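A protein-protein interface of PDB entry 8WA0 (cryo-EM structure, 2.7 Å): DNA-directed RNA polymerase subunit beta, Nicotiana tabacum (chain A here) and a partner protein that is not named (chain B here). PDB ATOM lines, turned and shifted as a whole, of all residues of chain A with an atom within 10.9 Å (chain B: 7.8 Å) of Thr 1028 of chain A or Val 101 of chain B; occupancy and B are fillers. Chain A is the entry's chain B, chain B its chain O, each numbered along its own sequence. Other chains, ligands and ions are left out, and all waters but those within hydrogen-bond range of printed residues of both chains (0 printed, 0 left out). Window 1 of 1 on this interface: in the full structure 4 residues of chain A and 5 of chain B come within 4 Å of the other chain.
Among the printed residues, merely in contact across the chains: Ile 1025 of chain A with Arg 105 of chain B (3.7 Å), Gly 1026 of chain A with Val 101 of chain B (3.97 Å), Gly 1026 of chain A with Arg 105 of chain B (3.6 Å), Thr 1028 of chain A with Lys 98 of chain B (3.6 Å) and Thr 1028 of chain A with Val 101 of chain B (3.5 Å).
The side-chain amino group of Lys 98 of chain B is in salt-bridge range of the side-chain carboxylate of Glu 102 of chain B, at 3.3 Å.
The side-chain hydroxyl (OG1) of Thr 1028 of chain A sits at hydrogen-bond distance from the side-chain carboxylate (OE1) of Glu 102 of chain B.
Printed residues of chain B within 4 Å of Ile 1025 of chain A: Arg 105.
Of the printed residues of chain B, Gly 1026 of chain A touches Val 101 (3.97 Å) and Arg 105 (3.6 Å).
No residue of chain B comes within 4 Å of Gly 1027 of chain A.
Of chain B, only Lys 98 (3.6 Å), Val 101 (3.5 Å) and Glu 102 (2.9 Å) come within 4 Å of Thr 1028 of chain A.
Lys 98 of chain B touches just one residue of chain A: Thr 1028.
Tyr 100 of chain B touches none of the printed residues of chain A.
No residue of chain A comes within 4 Å of Asn 103 of chain B.
The nearest printed residue of chain B that does not touch Ile 1025 of chain A is Asp 106 of chain B (6.9 Å).
Hydrophobic or aromatic side chains of chain B within 4 Å of the printed part of chain A: Val 101.
Hydrophobic or aromatic side chains of chain A within 4 Å of the printed part of chain B: Ile 1025.
Among the printed residues, 6 pairs touch across the chains.
Among the printed residues, no Asp or Glu carboxylate lies within 4 Å of a Lys or Arg side-chain nitrogen of the other chain.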
ATOM      1  N   GLU A1004     -13.632  25.701   6.820  1.00  0.00           N
ATOM      2  CA  GLU A1004     -12.582  25.293   5.908  1.00  0.00           C
ATOM      3  C   GLU A1004     -11.724  26.447   5.502  1.00  0.00           C
ATOM      4  O   GLU A1004     -10.513  26.353   5.495  1.00  0.00           O
ATOM      5  CB  GLU A1004     -13.215  24.721   4.662  1.00  0.00           C
ATOM      6  CG  GLU A1004     -12.398  23.674   3.947  1.00  0.00           C
ATOM      7  CD  GLU A1004     -13.108  23.179   2.711  1.00  0.00           C
ATOM      8  OE1 GLU A1004     -13.036  21.971   2.433  1.00  0.00           O
ATOM      9  OE2 GLU A1004     -13.753  24.001   2.032  1.00  0.00           O
ATOM     10  N   TYR A1008      -8.023  24.785   7.060  1.00  0.00           N
ATOM     11  CA  TYR A1008      -7.224  24.007   6.131  1.00  0.00           C
ATOM     12  C   TYR A1008      -6.611  24.833   5.038  1.00  0.00           C
ATOM     13  O   TYR A1008      -5.445  24.670   4.714  1.00  0.00           O
ATOM     14  CB  TYR A1008      -8.130  22.999   5.443  1.00  0.00           C
ATOM     15  CG  TYR A1008      -8.352  21.764   6.225  1.00  0.00           C
ATOM     16  CD1 TYR A1008      -7.281  21.060   6.693  1.00  0.00           C
ATOM     17  CD2 TYR A1008      -9.622  21.288   6.489  1.00  0.00           C
ATOM     18  CE1 TYR A1008      -7.443  19.901   7.405  1.00  0.00           C
ATOM     19  CE2 TYR A1008      -9.794  20.127   7.217  1.00  0.00           C
ATOM     20  CZ  TYR A1008      -8.681  19.445   7.675  1.00  0.00           C
ATOM     21  OH  TYR A1008      -8.737  18.286   8.406  1.00  0.00           O
ATOM     22  N   ALA A1015      -2.775  20.586   9.514  1.00  0.00           N
ATOM     23  CA  ALA A1015      -3.932  20.236   8.732  1.00  0.00           C
ATOM     24  C   ALA A1015      -3.722  20.458   7.264  1.00  0.00           C
ATOM     25  O   ALA A1015      -4.124  19.648   6.446  1.00  0.00           O
ATOM     26  CB  ALA A1015      -5.084  21.061   9.230  1.00  0.00           C
ATOM     27  N   GLU A1018      -1.828  17.727   5.384  1.00  0.00           N
ATOM     28  CA  GLU A1018      -2.567  16.497   5.191  1.00  0.00           C
ATOM     29  C   GLU A1018      -3.506  16.495   4.003  1.00  0.00           C
ATOM     30  O   GLU A1018      -3.550  15.527   3.260  1.00  0.00           O
ATOM     31  CB  GLU A1018      -3.367  16.194   6.441  1.00  0.00           C
ATOM     32  CG  GLU A1018      -2.529  15.992   7.686  1.00  0.00           C
ATOM     33  CD  GLU A1018      -3.331  16.194   8.955  1.00  0.00           C
ATOM     34  OE1 GLU A1018      -2.766  16.020  10.053  1.00  0.00           O
ATOM     35  OE2 GLU A1018      -4.528  16.531   8.852  1.00  0.00           O
ATOM     36  N   VAL A1019      -4.280  17.553   3.835  1.00  0.00           N
ATOM     37  CA  VAL A1019      -5.253  17.613   2.759  1.00  0.00           C
ATOM     38  C   VAL A1019      -4.651  17.362   1.397  1.00  0.00           C
ATOM     39  O   VAL A1019      -5.312  16.778   0.557  1.00  0.00           O
ATOM     40  CB  VAL A1019      -6.098  18.903   2.761  1.00  0.00           C
ATOM     41  CG1 VAL A1019      -6.708  19.141   4.126  1.00  0.00           C
ATOM     42  CG2 VAL A1019      -5.314  20.113   2.291  1.00  0.00           C
ATOM     43  N   LEU A1020      -3.432  17.795   1.132  1.00  0.00           N
ATOM     44  CA  LEU A1020      -2.904  17.513  -0.170  1.00  0.00           C
ATOM     45  C   LEU A1020      -2.835  16.008  -0.354  1.00  0.00           C
ATOM     46  O   LEU A1020      -3.233  15.501  -1.394  1.00  0.00           O
ATOM     47  CB  LEU A1020      -1.553  18.168  -0.331  1.00  0.00           C
ATOM     48  CG  LEU A1020      -0.766  17.921  -1.614  1.00  0.00           C
ATOM     49  CD1 LEU A1020      -1.519  18.450  -2.820  1.00  0.00           C
ATOM     50  CD2 LEU A1020       0.600  18.576  -1.514  1.00  0.00           C
ATOM     51  N   GLY A1021      -2.394  15.272   0.657  1.00  0.00           N
ATOM     52  CA  GLY A1021      -2.400  13.833   0.579  1.00  0.00           C
ATOM     53  C   GLY A1021      -3.739  13.121   0.467  1.00  0.00           C
ATOM     54  O   GLY A1021      -3.875  12.236  -0.355  1.00  0.00           O
ATOM     55  N   THR A1022      -4.704  13.475   1.296  1.00  0.00           N
ATOM     56  CA  THR A1022      -5.997  12.838   1.213  1.00  0.00           C
ATOM     57  C   THR A1022      -6.504  12.934  -0.198  1.00  0.00           C
ATOM     58  O   THR A1022      -7.002  11.963  -0.742  1.00  0.00           O
ATOM     59  CB  THR A1022      -7.028  13.499   2.129  1.00  0.00           C
ATOM     60  OG1 THR A1022      -7.186  14.871   1.760  1.00  0.00           O
ATOM     61  CG2 THR A1022      -6.583  13.423   3.573  1.00  0.00           C
ATOM     62  N   THR A1023      -6.380  14.105  -0.802  1.00  0.00           N
ATOM     63  CA  THR A1023      -6.917  14.306  -2.136  1.00  0.00           C
ATOM     64  C   THR A1023      -6.261  13.448  -3.215  1.00  0.00           C
ATOM     65  O   THR A1023      -6.944  12.912  -4.082  1.00  0.00           O
ATOM     66  CB  THR A1023      -6.867  15.785  -2.525  1.00  0.00           C
ATOM     67  OG1 THR A1023      -7.324  16.581  -1.427  1.00  0.00           O
ATOM     68  CG2 THR A1023      -7.749  16.047  -3.723  1.00  0.00           C
ATOM     69  N   ILE A1024      -4.946  13.301  -3.165  1.00  0.00           N
ATOM     70  CA  ILE A1024      -4.256  12.494  -4.157  1.00  0.00           C
ATOM     71  C   ILE A1024      -4.660  11.036  -4.000  1.00  0.00           C
ATOM     72  O   ILE A1024      -4.868  10.336  -4.984  1.00  0.00           O
ATOM     73  CB  ILE A1024      -2.737  12.650  -4.040  1.00  0.00           C
ATOM     74  CG1 ILE A1024      -2.347  14.109  -4.242  1.00  0.00           C
ATOM     75  CG2 ILE A1024      -2.021  11.791  -5.068  1.00  0.00           C
ATOM     76  CD1 ILE A1024      -0.862  14.363  -4.132  1.00  0.00           C
ATOM     77  N   ILE A1025      -4.793  10.575  -2.763  1.00  0.00           N
ATOM     78  CA  ILE A1025      -5.216   9.208  -2.515  1.00  0.00           C
ATOM     79  C   ILE A1025      -6.673   8.985  -2.834  1.00  0.00           C
ATOM     80  O   ILE A1025      -7.030   7.966  -3.392  1.00  0.00           O
ATOM     81  CB  ILE A1025      -4.899   8.861  -1.058  1.00  0.00           C
ATOM     82  CG1 ILE A1025      -3.391   8.898  -0.836  1.00  0.00           C
ATOM     83  CG2 ILE A1025      -5.460   7.505  -0.669  1.00  0.00           C
ATOM     84  CD1 ILE A1025      -2.988   8.577   0.584  1.00  0.00           C
ATOM     85  N   GLY A1026      -7.526   9.953  -2.541  1.00  0.00           N
ATOM     86  CA  GLY A1026      -8.959   9.752  -2.702  1.00  0.00           C
ATOM     87  C   GLY A1026      -9.783   9.620  -1.437  1.00  0.00           C
ATOM     88  O   GLY A1026     -10.908   9.176  -1.495  1.00  0.00           O
ATOM     89  N   GLY A1027      -9.230   9.992  -0.295  1.00  0.00           N
ATOM     90  CA  GLY A1027      -9.926   9.885   0.968  1.00  0.00           C
ATOM     91  C   GLY A1027     -10.859  10.972   1.453  1.00  0.00           C
ATOM     92  O   GLY A1027     -11.242  11.850   0.696  1.00  0.00           O
ATOM     93  N   THR A1028     -11.215  10.923   2.731  1.00  0.00           N
ATOM     94  CA  THR A1028     -12.100  11.923   3.309  1.00  0.00           C
ATOM     95  C   THR A1028     -11.327  12.833   4.250  1.00  0.00           C
ATOM     96  O   THR A1028     -10.407  12.384   4.922  1.00  0.00           O
ATOM     97  CB  THR A1028     -13.248  11.249   4.069  1.00  0.00           C
ATOM     98  OG1 THR A1028     -13.671  10.082   3.359  1.00  0.00           O
ATOM     99  CG2 THR A1028     -14.423  12.198   4.215  1.00  0.00           C
ATOM    100  N   ILE A1029     -11.699  14.106   4.318  1.00  0.00           N
ATOM    101  CA  ILE A1029     -10.957  15.055   5.130  1.00  0.00           C
ATOM    102  C   ILE A1029     -11.662  15.268   6.451  1.00  0.00           C
ATOM    103  O   ILE A1029     -12.830  15.635   6.477  1.00  0.00           O
ATOM    104  CB  ILE A1029     -10.847  16.408   4.411  1.00  0.00           C
ATOM    105  CG1 ILE A1029     -10.309  16.216   2.995  1.00  0.00           C
ATOM    106  CG2 ILE A1029      -9.965  17.369   5.189  1.00  0.00           C
ATOM    107  CD1 ILE A1029     -10.164  17.506   2.222  1.00  0.00           C
ATOM    108  N   PRO A1030     -10.951  15.037   7.561  1.00  0.00           N
ATOM    109  CA  PRO A1030     -11.570  15.181   8.878  1.00  0.00           C
ATOM    110  C   PRO A1030     -11.700  16.636   9.314  1.00  0.00           C
ATOM    111  O   PRO A1030     -11.010  17.490   8.770  1.00  0.00           O
ATOM    112  CB  PRO A1030     -10.607  14.439   9.790  1.00  0.00           C
ATOM    113  CG  PRO A1030      -9.289  14.534   9.106  1.00  0.00           C
ATOM    114  CD  PRO A1030      -9.588  14.486   7.640  1.00  0.00           C
ATOM    115  N   ASN A1031     -12.566  16.914  10.280  1.00  0.00           N
ATOM    116  CA  ASN A1031     -12.777  18.278  10.743  1.00  0.00           C
ATOM    117  C   ASN A1031     -11.752  18.567  11.779  1.00  0.00           C
ATOM    118  O   ASN A1031     -11.580  17.785  12.701  1.00  0.00           O
ATOM    119  CB  ASN A1031     -14.155  18.434  11.367  1.00  0.00           C
ATOM    120  CG  ASN A1031     -15.264  18.482  10.341  1.00  0.00           C
ATOM    121  OD1 ASN A1031     -15.019  18.521   9.135  1.00  0.00           O
ATOM    122  ND2 ASN A1031     -16.503  18.485  10.818  1.00  0.00           N
ATOM    123  N   PRO A1032     -11.048  19.685  11.646  1.00  0.00           N
ATOM    124  CA  PRO A1032      -9.960  19.990  12.576  1.00  0.00           C
ATOM    125  C   PRO A1032     -10.341  20.303  14.035  1.00  0.00           C
ATOM    126  O   PRO A1032     -11.366  20.918  14.289  1.00  0.00           O
ATOM    127  CB  PRO A1032      -9.309  21.209  11.937  1.00  0.00           C
ATOM    128  CG  PRO A1032      -9.752  21.212  10.521  1.00  0.00           C
ATOM    129  CD  PRO A1032     -11.132  20.660  10.553  1.00  0.00           C
ATOM    130  N   ALA B  94     -24.524  14.272   3.776  1.00  0.00           N
ATOM    131  CA  ALA B  94     -23.092  14.256   3.950  1.00  0.00           C
ATOM    132  C   ALA B  94     -22.581  13.039   4.615  1.00  0.00           C
ATOM    133  O   ALA B  94     -21.578  12.497   4.198  1.00  0.00           O
ATOM    134  CB  ALA B  94     -22.685  15.454   4.712  1.00  0.00           C
ATOM    135  N   ALA B  95     -23.252  12.564   5.630  1.00  0.00           N
ATOM    136  CA  ALA B  95     -22.908  11.328   6.252  1.00  0.00           C
ATOM    137  C   ALA B  95     -23.015  10.108   5.392  1.00  0.00           C
ATOM    138  O   ALA B  95     -22.143   9.269   5.438  1.00  0.00           O
ATOM    139  CB  ALA B  95     -23.766  11.139   7.435  1.00  0.00           C
ATOM    140  N   GLU B  96     -24.035   9.982   4.581  1.00  0.00           N
ATOM    141  CA  GLU B  96     -24.144   8.859   3.699  1.00  0.00           C
ATOM    142  C   GLU B  96     -23.058   8.820   2.693  1.00  0.00           C
ATOM    143  O   GLU B  96     -22.565   7.758   2.369  1.00  0.00           O
ATOM    144  CB  GLU B  96     -25.484   8.813   3.040  1.00  0.00           C
ATOM    145  CG  GLU B  96     -26.006   7.427   2.769  1.00  0.00           C
ATOM    146  CD  GLU B  96     -27.453   7.449   2.345  1.00  0.00           C
ATOM    147  OE1 GLU B  96     -28.086   8.513   2.480  1.00  0.00           O
ATOM    148  OE2 GLU B  96     -27.959   6.406   1.883  1.00  0.00           O
ATOM    149  N   ALA B  97     -22.662   9.956   2.181  1.00  0.00           N
ATOM    150  CA  ALA B  97     -21.608  10.023   1.221  1.00  0.00           C
ATOM    151  C   ALA B  97     -20.315   9.590   1.782  1.00  0.00           C
ATOM    152  O   ALA B  97     -19.553   8.918   1.113  1.00  0.00           O
ATOM    153  CB  ALA B  97     -21.508  11.398   0.652  1.00  0.00           C
ATOM    154  N   LYS B  98     -20.037   9.936   3.002  1.00  0.00           N
ATOM    155  CA  LYS B  98     -18.844   9.482   3.640  1.00  0.00           C
ATOM    156  C   LYS B  98     -18.806   7.988   3.814  1.00  0.00           C
ATOM    157  O   LYS B  98     -17.772   7.380   3.613  1.00  0.00           O
ATOM    158  CB  LYS B  98     -18.653  10.218   4.933  1.00  0.00           C
ATOM    159  CG  LYS B  98     -17.385   9.882   5.687  1.00  0.00           C
ATOM    160  CD  LYS B  98     -17.166  10.853   6.834  1.00  0.00           C
ATOM    161  CE  LYS B  98     -16.086  10.346   7.774  1.00  0.00           C
ATOM    162  NZ  LYS B  98     -14.829  10.003   7.054  1.00  0.00           N
ATOM    163  N   GLN B  99     -19.907   7.363   4.156  1.00  0.00           N
ATOM    164  CA  GLN B  99     -19.923   5.933   4.262  1.00  0.00           C
ATOM    165  C   GLN B  99     -19.665   5.271   2.978  1.00  0.00           C
ATOM    166  O   GLN B  99     -18.930   4.303   2.922  1.00  0.00           O
ATOM    167  CB  GLN B  99     -21.195   5.421   4.832  1.00  0.00           C
ATOM    168  CG  GLN B  99     -21.525   5.976   6.201  1.00  0.00           C
ATOM    169  CD  GLN B  99     -23.020   6.096   6.422  1.00  0.00           C
ATOM    170  OE1 GLN B  99     -23.469   6.539   7.478  1.00  0.00           O
ATOM    171  NE2 GLN B  99     -23.797   5.705   5.419  1.00  0.00           N
ATOM    172  N   TYR B 100     -20.223   5.775   1.919  1.00  0.00           N
ATOM    173  CA  TYR B 100     -19.965   5.220   0.625  1.00  0.00           C
ATOM    174  C   TYR B 100     -18.517   5.321   0.181  1.00  0.00           C
ATOM    175  O   TYR B 100     -17.970   4.348  -0.314  1.00  0.00           O
ATOM    176  CB  TYR B 100     -20.866   5.816  -0.434  1.00  0.00           C
ATOM    177  CG  TYR B 100     -22.342   5.545  -0.361  1.00  0.00           C
ATOM    178  CD1 TYR B 100     -22.911   4.855   0.691  1.00  0.00           C
ATOM    179  CD2 TYR B 100     -23.172   5.997  -1.360  1.00  0.00           C
ATOM    180  CE1 TYR B 100     -24.271   4.630   0.734  1.00  0.00           C
ATOM    181  CE2 TYR B 100     -24.523   5.771  -1.325  1.00  0.00           C
ATOM    182  CZ  TYR B 100     -25.066   5.092  -0.285  1.00  0.00           C
ATOM    183  OH  TYR B 100     -26.420   4.874  -0.261  1.00  0.00           O
ATOM    184  N   VAL B 101     -17.833   6.405   0.451  1.00  0.00           N
ATOM    185  CA  VAL B 101     -16.474   6.556   0.016  1.00  0.00           C
ATOM    186  C   VAL B 101     -15.563   5.776   0.896  1.00  0.00           C
ATOM    187  O   VAL B 101     -14.592   5.215   0.424  1.00  0.00           O
ATOM    188  CB  VAL B 101     -16.025   8.020  -0.162  1.00  0.00           C
ATOM    189  CG1 VAL B 101     -16.008   8.768   1.155  1.00  0.00           C
ATOM    190  CG2 VAL B 101     -14.682   8.111  -0.854  1.00  0.00           C
ATOM    191  N   GLU B 102     -15.862   5.666   2.163  1.00  0.00           N
ATOM    192  CA  GLU B 102     -15.054   4.832   2.985  1.00  0.00           C
ATOM    193  C   GLU B 102     -15.113   3.388   2.598  1.00  0.00           C
ATOM    194  O   GLU B 102     -14.087   2.740   2.521  1.00  0.00           O
ATOM    195  CB  GLU B 102     -15.452   4.968   4.427  1.00  0.00           C
ATOM    196  CG  GLU B 102     -14.368   5.561   5.308  1.00  0.00           C
ATOM    197  CD  GLU B 102     -14.032   6.997   4.951  1.00  0.00           C
ATOM    198  OE1 GLU B 102     -14.955   7.759   4.595  1.00  0.00           O
ATOM    199  OE2 GLU B 102     -12.844   7.371   5.041  1.00  0.00           O
ATOM    200  N   ASN B 103     -16.283   2.854   2.342  1.00  0.00           N
ATOM    201  CA  ASN B 103     -16.376   1.483   1.881  1.00  0.00           C
ATOM    202  C   ASN B 103     -15.803   1.090   0.515  1.00  0.00           C
ATOM    203  O   ASN B 103     -15.165   0.056   0.421  1.00  0.00           O
ATOM    204  CB  ASN B 103     -17.766   0.951   2.055  1.00  0.00           C
ATOM    205  CG  ASN B 103     -18.272   1.114   3.465  1.00  0.00           C
ATOM    206  OD1 ASN B 103     -17.497   1.339   4.392  1.00  0.00           O
ATOM    207  ND2 ASN B 103     -19.583   1.001   3.640  1.00  0.00           N
ATOM    208  N   ASN B 104     -15.986   1.862  -0.533  1.00  0.00           N
ATOM    209  CA  ASN B 104     -15.388   1.565  -1.816  1.00  0.00           C
ATOM    210  C   ASN B 104     -14.712   2.774  -2.379  1.00  0.00           C
ATOM    211  O   ASN B 104     -15.306   3.476  -3.176  1.00  0.00           O
ATOM    212  CB  ASN B 104     -16.437   1.082  -2.772  1.00  0.00           C
ATOM    213  CG  ASN B 104     -15.853   0.399  -3.987  1.00  0.00           C
ATOM    214  OD1 ASN B 104     -16.515   0.275  -5.017  1.00  0.00           O
ATOM    215  ND2 ASN B 104     -14.607  -0.047  -3.879  1.00  0.00           N
ATOM    216  N   ARG B 105     -13.483   3.044  -1.997  1.00  0.00           N
ATOM    217  CA  ARG B 105     -12.809   4.266  -2.404  1.00  0.00           C
ATOM    218  C   ARG B 105     -12.555   4.474  -3.844  1.00  0.00           C
ATOM    219  O   ARG B 105     -12.723   5.575  -4.342  1.00  0.00           O
ATOM    220  CB  ARG B 105     -11.488   4.388  -1.669  1.00  0.00           C
ATOM    221  CG  ARG B 105     -10.678   5.635  -1.930  1.00  0.00           C
ATOM    222  CD  ARG B 105      -9.549   5.710  -0.931  1.00  0.00           C
ATOM    223  NE  ARG B 105     -10.061   5.560   0.423  1.00  0.00           N
ATOM    224  CZ  ARG B 105      -9.314   5.627   1.518  1.00  0.00           C
ATOM    225  NH1 ARG B 105      -8.010   5.843   1.419  1.00  0.00           N
ATOM    226  NH2 ARG B 105      -9.870   5.480   2.711  1.00  0.00           N
ATOM    227  N   ASP B 106     -12.178   3.443  -4.553  1.00  0.00           N
ATOM    228  CA  ASP B 106     -11.778   3.624  -5.925  1.00  0.00           C
ATOM    229  C   ASP B 106     -12.830   3.746  -6.984  1.00  0.00           C
ATOM    230  O   ASP B 106     -12.492   4.039  -8.120  1.00  0.00           O
ATOM    231  CB  ASP B 106     -10.784   2.548  -6.304  1.00  0.00           C
ATOM    232  N   GLU B 107     -14.085   3.538  -6.668  1.00  0.00           N
ATOM    233  CA  GLU B 107     -15.119   3.741  -7.642  1.00  0.00           C
ATOM    234  C   GLU B 107     -15.220   5.182  -7.961  1.00  0.00           C
ATOM    235  O   GLU B 107     -15.387   5.550  -9.109  1.00  0.00           O
ATOM    236  CB  GLU B 107     -16.443   3.252  -7.092  1.00  0.00           C
ATOM    237  N   TYR B 108     -15.113   6.023  -6.959  1.00  0.00           N
ATOM    238  CA  TYR B 108     -15.299   7.433  -7.147  1.00  0.00           C
ATOM    239  C   TYR B 108     -14.171   8.249  -7.702  1.00  0.00           C
ATOM    240  O   TYR B 108     -13.027   7.837  -7.643  1.00  0.00           O
ATOM    241  CB  TYR B 108     -15.850   8.008  -5.870  1.00  0.00           C
ATOM    242  CG  TYR B 108     -17.010   7.231  -5.324  1.00  0.00           C
ATOM    243  CD1 TYR B 108     -18.208   7.167  -6.004  1.00  0.00           C
ATOM    244  CD2 TYR B 108     -16.907   6.562  -4.126  1.00  0.00           C
ATOM    245  CE1 TYR B 108     -19.270   6.450  -5.508  1.00  0.00           C
ATOM    246  CE2 TYR B 108     -17.965   5.845  -3.622  1.00  0.00           C
ATOM    247  CZ  TYR B 108     -19.139   5.796  -4.321  1.00  0.00           C
ATOM    248  OH  TYR B 108     -20.191   5.083  -3.823  1.00  0.00           O
ATOM    249  N   GLY B 109     -14.482   9.420  -8.233  1.00  0.00           N
ATOM    250  CA  GLY B 109     -13.499  10.287  -8.852  1.00  0.00           C
ATOM    251  C   GLY B 109     -14.072  10.965 -10.070  1.00  0.00           C
ATOM    252  O   GLY B 109     -13.860  12.147 -10.265  1.00  0.00           O
ATOM    253  N   ALA B 113     -19.823  10.874  -5.109  1.00  0.00           N
ATOM    254  CA  ALA B 113     -20.617  10.263  -4.084  1.00  0.00           C
ATOM    255  C   ALA B 113     -21.910  10.947  -3.722  1.00  0.00           C
ATOM    256  O   ALA B 113     -22.883  10.277  -3.454  1.00  0.00           O
ATOM    257  CB  ALA B 113     -19.760  10.070  -2.881  1.00  0.00           C
